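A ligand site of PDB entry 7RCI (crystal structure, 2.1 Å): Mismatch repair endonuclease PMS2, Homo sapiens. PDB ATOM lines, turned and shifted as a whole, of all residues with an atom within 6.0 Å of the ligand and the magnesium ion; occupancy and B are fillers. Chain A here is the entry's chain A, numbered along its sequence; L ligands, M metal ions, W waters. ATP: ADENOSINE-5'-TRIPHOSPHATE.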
ATOM      1  N   GLU A  41      -6.747  12.163  -6.736  1.00  0.00           N
ATOM      2  CA  GLU A  41      -8.037  11.750  -7.278  1.00  0.00           C
ATOM      3  C   GLU A  41      -9.062  12.875  -7.213  1.00  0.00           C
ATOM      4  O   GLU A  41      -9.839  13.062  -8.156  1.00  0.00           O
ATOM      5  CB  GLU A  41      -8.537  10.513  -6.539  1.00  0.00           C
ATOM      6  CG  GLU A  41      -7.576   9.339  -6.554  1.00  0.00           C
ATOM      7  CD  GLU A  41      -7.665   8.505  -7.812  1.00  0.00           C
ATOM      8  OE1 GLU A  41      -8.508   8.814  -8.689  1.00  0.00           O
ATOM      9  OE2 GLU A  41      -6.889   7.534  -7.943  1.00  0.00           O
ATOM     10  N   LEU A  42      -9.074  13.638  -6.120  1.00  0.00           N
ATOM     11  CA  LEU A  42     -10.014  14.750  -6.008  1.00  0.00           C
ATOM     12  C   LEU A  42      -9.709  15.835  -7.040  1.00  0.00           C
ATOM     13  O   LEU A  42     -10.638  16.469  -7.557  1.00  0.00           O
ATOM     14  CB  LEU A  42      -9.985  15.347  -4.606  1.00  0.00           C
ATOM     15  CG  LEU A  42     -10.584  14.499  -3.481  1.00  0.00           C
ATOM     16  CD1 LEU A  42     -10.510  15.244  -2.158  1.00  0.00           C
ATOM     17  CD2 LEU A  42     -12.022  14.137  -3.806  1.00  0.00           C
ATOM     18  N   GLU A  44      -8.258  15.212  -9.992  1.00  0.00           N
ATOM     19  CA  GLU A  44      -8.680  14.618 -11.264  1.00  0.00           C
ATOM     20  C   GLU A  44     -10.173  14.790 -11.478  1.00  0.00           C
ATOM     21  O   GLU A  44     -10.618  15.064 -12.605  1.00  0.00           O
ATOM     22  CB  GLU A  44      -8.302  13.143 -11.311  1.00  0.00           C
ATOM     23  CG  GLU A  44      -6.817  12.858 -11.430  1.00  0.00           C
ATOM     24  CD  GLU A  44      -6.296  13.045 -12.838  1.00  0.00           C
ATOM     25  OE1 GLU A  44      -7.134  13.117 -13.766  1.00  0.00           O
ATOM     26  OE2 GLU A  44      -5.071  13.109 -13.021  1.00  0.00           O
ATOM     27  N   ASN A  45     -10.967  14.614 -10.421  1.00  0.00           N
ATOM     28  CA  ASN A  45     -12.408  14.780 -10.540  1.00  0.00           C
ATOM     29  C   ASN A  45     -12.782  16.208 -10.928  1.00  0.00           C
ATOM     30  O   ASN A  45     -13.701  16.422 -11.721  1.00  0.00           O
ATOM     31  CB  ASN A  45     -13.089  14.383  -9.236  1.00  0.00           C
ATOM     32  CG  ASN A  45     -12.990  12.901  -8.955  1.00  0.00           C
ATOM     33  OD1 ASN A  45     -12.715  12.099  -9.856  1.00  0.00           O
ATOM     34  ND2 ASN A  45     -13.215  12.515  -7.704  1.00  0.00           N
ATOM     35  N   SER A  46     -12.072  17.189 -10.368  1.00  0.00           N
ATOM     36  CA  SER A  46     -12.343  18.579 -10.716  1.00  0.00           C
ATOM     37  C   SER A  46     -11.923  18.881 -12.157  1.00  0.00           C
ATOM     38  O   SER A  46     -12.633  19.585 -12.876  1.00  0.00           O
ATOM     39  CB  SER A  46     -11.633  19.517  -9.742  1.00  0.00           C
ATOM     40  OG  SER A  46     -12.066  19.286  -8.417  1.00  0.00           O
ATOM     41  N   ASP A  48     -11.751  16.714 -14.664  1.00  0.00           N
ATOM     42  CA  ASP A  48     -12.678  16.037 -15.562  1.00  0.00           C
ATOM     43  C   ASP A  48     -14.017  16.764 -15.649  1.00  0.00           C
ATOM     44  O   ASP A  48     -14.697  16.668 -16.676  1.00  0.00           O
ATOM     45  CB  ASP A  48     -12.899  14.603 -15.090  1.00  0.00           C
ATOM     46  CG  ASP A  48     -11.635  13.769 -15.159  1.00  0.00           C
ATOM     47  OD1 ASP A  48     -10.623  14.262 -15.685  1.00  0.00           O
ATOM     48  OD2 ASP A  48     -11.665  12.614 -14.677  1.00  0.00           O
ATOM     49  N   ALA A  49     -14.392  17.487 -14.596  1.00  0.00           N
ATOM     50  CA  ALA A  49     -15.626  18.262 -14.595  1.00  0.00           C
ATOM     51  C   ALA A  49     -15.526  19.544 -15.412  1.00  0.00           C
ATOM     52  O   ALA A  49     -16.514  20.282 -15.496  1.00  0.00           O
ATOM     53  CB  ALA A  49     -16.035  18.584 -13.157  1.00  0.00           C
ATOM     54  N   ASP A  70     -14.231  23.260  -6.522  1.00  0.00           N
ATOM     55  CA  ASP A  70     -14.096  23.631  -7.929  1.00  0.00           C
ATOM     56  C   ASP A  70     -15.395  24.255  -8.405  1.00  0.00           C
ATOM     57  O   ASP A  70     -16.437  24.181  -7.755  1.00  0.00           O
ATOM     58  CB  ASP A  70     -13.720  22.418  -8.797  1.00  0.00           C
ATOM     59  CG  ASP A  70     -14.811  21.361  -8.833  1.00  0.00           C
ATOM     60  OD1 ASP A  70     -15.799  21.542  -9.561  1.00  0.00           O
ATOM     61  OD2 ASP A  70     -14.654  20.338  -8.123  1.00  0.00           O
ATOM     62  N   GLY A  72     -16.649  23.396 -11.483  1.00  0.00           N
ATOM     63  CA  GLY A  72     -16.907  22.544 -12.627  1.00  0.00           C
ATOM     64  C   GLY A  72     -18.381  22.337 -12.883  1.00  0.00           C
ATOM     65  O   GLY A  72     -19.237  23.119 -12.450  1.00  0.00           O
ATOM     66  N   CYS A  73     -18.692  21.250 -13.595  1.00  0.00           N
ATOM     67  CA  CYS A  73     -20.061  20.996 -14.020  1.00  0.00           C
ATOM     68  C   CYS A  73     -20.994  20.642 -12.867  1.00  0.00           C
ATOM     69  O   CYS A  73     -22.202  20.844 -12.991  1.00  0.00           O
ATOM     70  CB  CYS A  73     -20.088  19.876 -15.069  1.00  0.00           C
ATOM     71  SG  CYS A  73     -19.425  18.291 -14.508  1.00  0.00           S
ATOM     72  N   GLY A  74     -20.464  20.122 -11.773  1.00  0.00           N
ATOM     73  CA  GLY A  74     -21.306  19.666 -10.685  1.00  0.00           C
ATOM     74  C   GLY A  74     -21.924  18.325 -11.005  1.00  0.00           C
ATOM     75  O   GLY A  74     -21.679  17.714 -12.046  1.00  0.00           O
ATOM     76  N   VAL A  75     -22.776  17.867 -10.091  1.00  0.00           N
ATOM     77  CA  VAL A  75     -23.434  16.575 -10.198  1.00  0.00           C
ATOM     78  C   VAL A  75     -24.934  16.799 -10.204  1.00  0.00           C
ATOM     79  O   VAL A  75     -25.458  17.562  -9.389  1.00  0.00           O
ATOM     80  CB  VAL A  75     -23.024  15.632  -9.053  1.00  0.00           C
ATOM     81  CG1 VAL A  75     -23.594  14.239  -9.276  1.00  0.00           C
ATOM     82  CG2 VAL A  75     -21.499  15.583  -8.921  1.00  0.00           C
ATOM     83  N   GLY A  82     -25.484   7.583  -7.029  1.00  0.00           N
ATOM     84  CA  GLY A  82     -24.438   6.946  -7.820  1.00  0.00           C
ATOM     85  C   GLY A  82     -23.030   7.453  -7.584  1.00  0.00           C
ATOM     86  O   GLY A  82     -22.092   6.924  -8.192  1.00  0.00           O
ATOM     87  N   LEU A  83     -22.854   8.465  -6.745  1.00  0.00           N
ATOM     88  CA  LEU A  83     -21.520   9.021  -6.509  1.00  0.00           C
ATOM     89  C   LEU A  83     -20.577   7.984  -5.904  1.00  0.00           C
ATOM     90  O   LEU A  83     -19.357   8.055  -6.126  1.00  0.00           O
ATOM     91  CB  LEU A  83     -21.607  10.245  -5.597  1.00  0.00           C
ATOM     92  CG  LEU A  83     -22.062  11.538  -6.260  1.00  0.00           C
ATOM     93  CD1 LEU A  83     -22.215  12.623  -5.213  1.00  0.00           C
ATOM     94  CD2 LEU A  83     -21.055  11.963  -7.326  1.00  0.00           C
ATOM     95  N   THR A  84     -21.107   7.014  -5.176  1.00  0.00           N
ATOM     96  CA  THR A  84     -20.293   6.015  -4.483  1.00  0.00           C
ATOM     97  C   THR A  84     -20.584   4.592  -4.939  1.00  0.00           C
ATOM     98  O   THR A  84     -20.037   3.653  -4.359  1.00  0.00           O
ATOM     99  CB  THR A  84     -20.495   6.129  -2.964  1.00  0.00           C
ATOM    100  OG1 THR A  84     -21.883   5.980  -2.652  1.00  0.00           O
ATOM    101  CG2 THR A  84     -20.010   7.480  -2.459  1.00  0.00           C
ATOM    102  N   ASP A  97      -4.971   4.985 -19.349  1.00  0.00           N
ATOM    103  CA  ASP A  97      -4.933   6.206 -18.538  1.00  0.00           C
ATOM    104  C   ASP A  97      -3.662   6.194 -17.711  1.00  0.00           C
ATOM    105  O   ASP A  97      -3.411   5.240 -16.958  1.00  0.00           O
ATOM    106  CB  ASP A  97      -6.171   6.310 -17.636  1.00  0.00           C
ATOM    107  CG  ASP A  97      -6.240   7.632 -16.861  1.00  0.00           C
ATOM    108  OD1 ASP A  97      -5.335   8.479 -17.008  1.00  0.00           O
ATOM    109  OD2 ASP A  97      -7.218   7.819 -16.104  1.00  0.00           O
ATOM    110  N   GLU A 109     -13.303   2.690  -7.171  1.00  0.00           N
ATOM    111  CA  GLU A 109     -13.443   4.121  -7.405  1.00  0.00           C
ATOM    112  C   GLU A 109     -13.073   4.898  -6.148  1.00  0.00           C
ATOM    113  O   GLU A 109     -13.339   4.457  -5.037  1.00  0.00           O
ATOM    114  CB  GLU A 109     -14.864   4.455  -7.874  1.00  0.00           C
ATOM    115  CG  GLU A 109     -15.288   3.683  -9.101  1.00  0.00           C
ATOM    116  CD  GLU A 109     -14.203   3.640 -10.164  1.00  0.00           C
ATOM    117  OE1 GLU A 109     -13.926   4.695 -10.786  1.00  0.00           O
ATOM    118  OE2 GLU A 109     -13.617   2.566 -10.383  1.00  0.00           O
ATOM    119  N   ALA A 110     -12.461   6.067  -6.350  1.00  0.00           N
ATOM    120  CA  ALA A 110     -11.882   6.809  -5.243  1.00  0.00           C
ATOM    121  C   ALA A 110     -12.926   7.231  -4.220  1.00  0.00           C
ATOM    122  O   ALA A 110     -12.721   7.086  -3.010  1.00  0.00           O
ATOM    123  CB  ALA A 110     -11.140   8.038  -5.771  1.00  0.00           C
ATOM    124  N   LEU A 111     -14.071   7.767  -4.685  1.00  0.00           N
ATOM    125  CA  LEU A 111     -15.051   8.313  -3.748  1.00  0.00           C
ATOM    126  C   LEU A 111     -15.611   7.227  -2.834  1.00  0.00           C
ATOM    127  O   LEU A 111     -15.847   7.484  -1.651  1.00  0.00           O
ATOM    128  CB  LEU A 111     -16.171   9.008  -4.523  1.00  0.00           C
ATOM    129  CG  LEU A 111     -15.867  10.420  -5.042  1.00  0.00           C
ATOM    130  CD1 LEU A 111     -17.119  11.040  -5.640  1.00  0.00           C
ATOM    131  CD2 LEU A 111     -15.298  11.294  -3.948  1.00  0.00           C
ATOM    132  N   SER A 112     -15.820   6.020  -3.359  1.00  0.00           N
ATOM    133  CA  SER A 112     -16.262   4.926  -2.495  1.00  0.00           C
ATOM    134  C   SER A 112     -15.172   4.527  -1.507  1.00  0.00           C
ATOM    135  O   SER A 112     -15.464   4.187  -0.361  1.00  0.00           O
ATOM    136  CB  SER A 112     -16.676   3.725  -3.340  1.00  0.00           C
ATOM    137  OG  SER A 112     -17.118   2.655  -2.522  1.00  0.00           O
ATOM    138  N   THR A 124     -22.685  20.365  -4.022  1.00  0.00           N
ATOM    139  CA  THR A 124     -22.539  20.516  -5.456  1.00  0.00           C
ATOM    140  C   THR A 124     -23.779  21.190  -6.034  1.00  0.00           C
ATOM    141  O   THR A 124     -24.832  21.250  -5.406  1.00  0.00           O
ATOM    142  CB  THR A 124     -22.326  19.170  -6.144  1.00  0.00           C
ATOM    143  OG1 THR A 124     -22.229  19.364  -7.561  1.00  0.00           O
ATOM    144  CG2 THR A 124     -23.492  18.241  -5.853  1.00  0.00           C
ATOM    145  N   GLY A 154     -20.661  23.832  -9.545  1.00  0.00           N
ATOM    146  CA  GLY A 154     -19.426  23.161  -9.193  1.00  0.00           C
ATOM    147  C   GLY A 154     -19.661  22.153  -8.103  1.00  0.00           C
ATOM    148  O   GLY A 154     -20.798  21.775  -7.814  1.00  0.00           O
ATOM    149  N   THR A 155     -18.569  21.720  -7.485  1.00  0.00           N
ATOM    150  CA  THR A 155     -18.604  20.684  -6.461  1.00  0.00           C
ATOM    151  C   THR A 155     -17.502  20.966  -5.444  1.00  0.00           C
ATOM    152  O   THR A 155     -16.413  21.424  -5.813  1.00  0.00           O
ATOM    153  CB  THR A 155     -18.409  19.289  -7.073  1.00  0.00           C
ATOM    154  OG1 THR A 155     -19.365  19.095  -8.123  1.00  0.00           O
ATOM    155  CG2 THR A 155     -18.596  18.208  -6.015  1.00  0.00           C
ATOM    156  N   THR A 156     -17.793  20.694  -4.180  1.00  0.00           N
ATOM    157  CA  THR A 156     -16.829  20.817  -3.095  1.00  0.00           C
ATOM    158  C   THR A 156     -16.823  19.507  -2.310  1.00  0.00           C
ATOM    159  O   THR A 156     -17.834  19.163  -1.680  1.00  0.00           O
ATOM    160  CB  THR A 156     -17.155  21.993  -2.180  1.00  0.00           C
ATOM    161  OG1 THR A 156     -17.247  23.192  -2.966  1.00  0.00           O
ATOM    162  CG2 THR A 156     -16.084  22.165  -1.131  1.00  0.00           C
ATOM    163  N   VAL A 157     -15.708  18.783  -2.345  1.00  0.00           N
ATOM    164  CA  VAL A 157     -15.569  17.505  -1.655  1.00  0.00           C
ATOM    165  C   VAL A 157     -14.654  17.713  -0.462  1.00  0.00           C
ATOM    166  O   VAL A 157     -13.493  18.132  -0.623  1.00  0.00           O
ATOM    167  CB  VAL A 157     -15.029  16.414  -2.582  1.00  0.00           C
ATOM    168  CG1 VAL A 157     -14.912  15.091  -1.837  1.00  0.00           C
ATOM    169  CG2 VAL A 157     -15.926  16.264  -3.797  1.00  0.00           C
HETATM  170  PG  ATP L   1     -11.613   7.063 -11.896  1.00  0.00           P
HETATM  171  O1G ATP L   1     -11.472   7.848 -10.625  1.00  0.00           O
HETATM  172  O2G ATP L   1     -10.797   7.720 -12.989  1.00  0.00           O
HETATM  173  O3G ATP L   1     -11.098   5.634 -11.674  1.00  0.00           O
HETATM  174  PB  ATP L   1     -14.440   7.958 -11.600  1.00  0.00           P
HETATM  175  O1B ATP L   1     -15.747   7.830 -12.327  1.00  0.00           O
HETATM  176  O2B ATP L   1     -13.995   9.416 -11.593  1.00  0.00           O
HETATM  177  O3B ATP L   1     -13.248   7.014 -12.353  1.00  0.00           O
HETATM  178  PA  ATP L   1     -14.687   8.459  -8.785  1.00  0.00           P
HETATM  179  O1A ATP L   1     -14.878   7.651  -7.432  1.00  0.00           O
HETATM  180  O2A ATP L   1     -13.439   9.206  -8.724  1.00  0.00           O
HETATM  181  O3A ATP L   1     -14.631   7.429 -10.013  1.00  0.00           O
HETATM  182  O5' ATP L   1     -16.001   9.535  -9.030  1.00  0.00           O
HETATM  183  C5' ATP L   1     -17.283   8.979  -9.108  1.00  0.00           C
HETATM  184  C4' ATP L   1     -18.229   9.949  -9.840  1.00  0.00           C
HETATM  185  O4' ATP L   1     -18.429  11.024  -9.109  1.00  0.00           O
HETATM  186  C3' ATP L   1     -17.565  10.450 -11.099  1.00  0.00           C
HETATM  187  O3' ATP L   1     -17.958   9.708 -12.149  1.00  0.00           O
HETATM  188  C2' ATP L   1     -18.100  11.910 -11.260  1.00  0.00           C
HETATM  189  O2' ATP L   1     -19.229  11.897 -12.205  1.00  0.00           O
HETATM  190  C1' ATP L   1     -18.513  12.282 -10.100  1.00  0.00           C
HETATM  191  N9  ATP L   1     -17.664  13.344  -9.564  1.00  0.00           N
HETATM  192  C8  ATP L   1     -16.719  13.114  -8.633  1.00  0.00           C
HETATM  193  N7  ATP L   1     -16.128  14.271  -8.360  1.00  0.00           N
HETATM  194  C5  ATP L   1     -16.699  15.241  -9.135  1.00  0.00           C
HETATM  195  C6  ATP L   1     -16.468  16.596  -9.253  1.00  0.00           C
HETATM  196  N6  ATP L   1     -15.545  17.516  -8.613  1.00  0.00           N
HETATM  197  N1  ATP L   1     -17.208  17.327 -10.117  1.00  0.00           N
HETATM  198  C2  ATP L   1     -18.152  16.743 -10.849  1.00  0.00           C
HETATM  199  N3  ATP L   1     -18.377  15.401 -10.729  1.00  0.00           N
HETATM  200  C4  ATP L   1     -17.642  14.657  -9.867  1.00  0.00           C
HETATM  201 MG    MG M   1     -12.086   9.812 -10.555  1.00  0.00          MG
HETATM  202  O   HOH W   1      -8.282   9.549 -11.579  1.00  0.00           O
HETATM  203  O   HOH W   2     -10.394  10.195  -9.447  1.00  0.00           O
HETATM  204  O   HOH W   3     -15.543  14.416 -12.418  1.00  0.00           O
HETATM  205  O   HOH W   4     -17.720  20.216 -10.310  1.00  0.00           O
HETATM  206  O   HOH W   5      -9.681   5.902 -15.413  1.00  0.00           O
HETATM  207  O   HOH W   6     -14.392  18.883  -5.640  1.00  0.00           O
HETATM  208  O   HOH W   7     -20.368  15.003 -13.159  1.00  0.00           O
HETATM  209  O   HOH W   8     -14.235  14.608  -6.175  1.00  0.00           O
HETATM  210  O   HOH W   9     -14.384  11.646 -13.233  1.00  0.00           O
HETATM  211  O   HOH W  10     -11.129  10.368 -12.308  1.00  0.00           O
HETATM  212  O   HOH W  11     -12.968  16.622  -6.581  1.00  0.00           O
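Water W2 is bound to the magnesium ion (2.1 Å).
The magnesium ion is bound by O1G of the ligand.
The magnesium ion is bound by water W10 (2.1 Å).
O2B of the ligand is bound to the magnesium ion (2.2 Å).
The magnesium ion is bound by O2A of the ligand, 2.4 Å away.
OD1 of Asn 45 is bound to the magnesium ion (2.5 Å).
The magnesium ion has six donor atoms within binding distance.
The backbone NH (N) of Asp 70 sits at hydrogen-bond distance from the backbone carbonyl oxygen (O) of Thr 155 (2.9 Å).
O of Ala 49 is in hydrogen-bond range of N of Cys 73 (3.0 Å).
The side-chain hydroxyl (OG1) of Thr 155 lies within hydrogen-bond range of the side-chain hydroxyl (OG1) of Thr 124 (2.9 Å).
The side-chain carboxylate of Asp 70 is in hydrogen-bond range of the backbone NH of Gly 72.
O of Leu 42 sits at hydrogen-bond distance from OG of Ser 46.
The backbone NH of Val 75 is in hydrogen-bond range of the side-chain hydroxyl of Thr 124.
The side-chain hydroxyl (OG) of Ser 46 lies within hydrogen-bond range of the side-chain carboxylate (OD2) of Asp 70 (2.8 Å).
The side-chain amide nitrogen of Asn 45 sits close to the backbone carbonyl oxygen of Glu 41, at 3.4 Å.
Of the 25 residues printed, 1 comes within 4 Å of the magnesium ion.
The side-chain carboxylate of Glu 109 sits close to an oxygen (O3B) of the ligand, 2.9 Å away.
Merely in contact with the ligand: Glu 41 (3.7 Å), Ser 46 (3.9 Å), Ala 49 (3.5 Å), Gly 74 (3.8 Å), Val 75 (3.6 Å) and Leu 83 (3.3 Å).
Hydrophobic or aromatic side chains that line the ligand: Ala 49, Val 75, Leu 83, Ala 110 and Leu 111.
Of the 25 residues printed, 12 come within 4 Å of the ligand.
The nearest printed residue that does not touch the ligand is Cys 73 (4.2 Å).
Water W4 lies within hydrogen-bond range of OD1 of Asp 70 (2.5 Å), N1 of the ligand (2.9 Å), OG1 of Thr 155 (3.0 Å) and N of Gly 74 (3.1 Å).
Water W7 lies within hydrogen-bond range of a nitrogen (N3) of the ligand (3.2 Å), the backbone carbonyl oxygen of Gly 74 (3.2 Å) and the side-chain sulfur of Cys 73 (3.7 Å).
Water W5 bridges OD2 of Asp 97 and O2G of the ligand.
Water W3 lies within hydrogen-bond range of the backbone carbonyl oxygen (O) of Asn 45 (2.8 Å) and a nitrogen (N3) of the ligand (3.4 Å).
Water W1 bridges the side-chain carboxylate of Glu 41 (3.0 Å) and an oxygen (O2G) of the ligand (3.4 Å).
Water W6 lies within hydrogen-bond range of the side-chain carboxylate (OD2) of Asp 70 (2.9 Å), the backbone carbonyl oxygen (O) of Thr 155 (3.3 Å) and a nitrogen (N6) of the ligand (3.5 Å).
The side-chain carboxylate of Asp 70 lies within hydrogen-bond range of a nitrogen (N6) of the ligand (3.0 Å).
The backbone NH of Leu 111 lies within hydrogen-bond range of an oxygen (O1A) of the ligand, 2.9 Å away.
The side-chain hydroxyl (OG1) of Thr 155 is in hydrogen-bond range of a nitrogen (N1) of the ligand (3.4 Å).
N of Ala 110 is in hydrogen-bond range of O1A of the ligand (3.1 Å).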
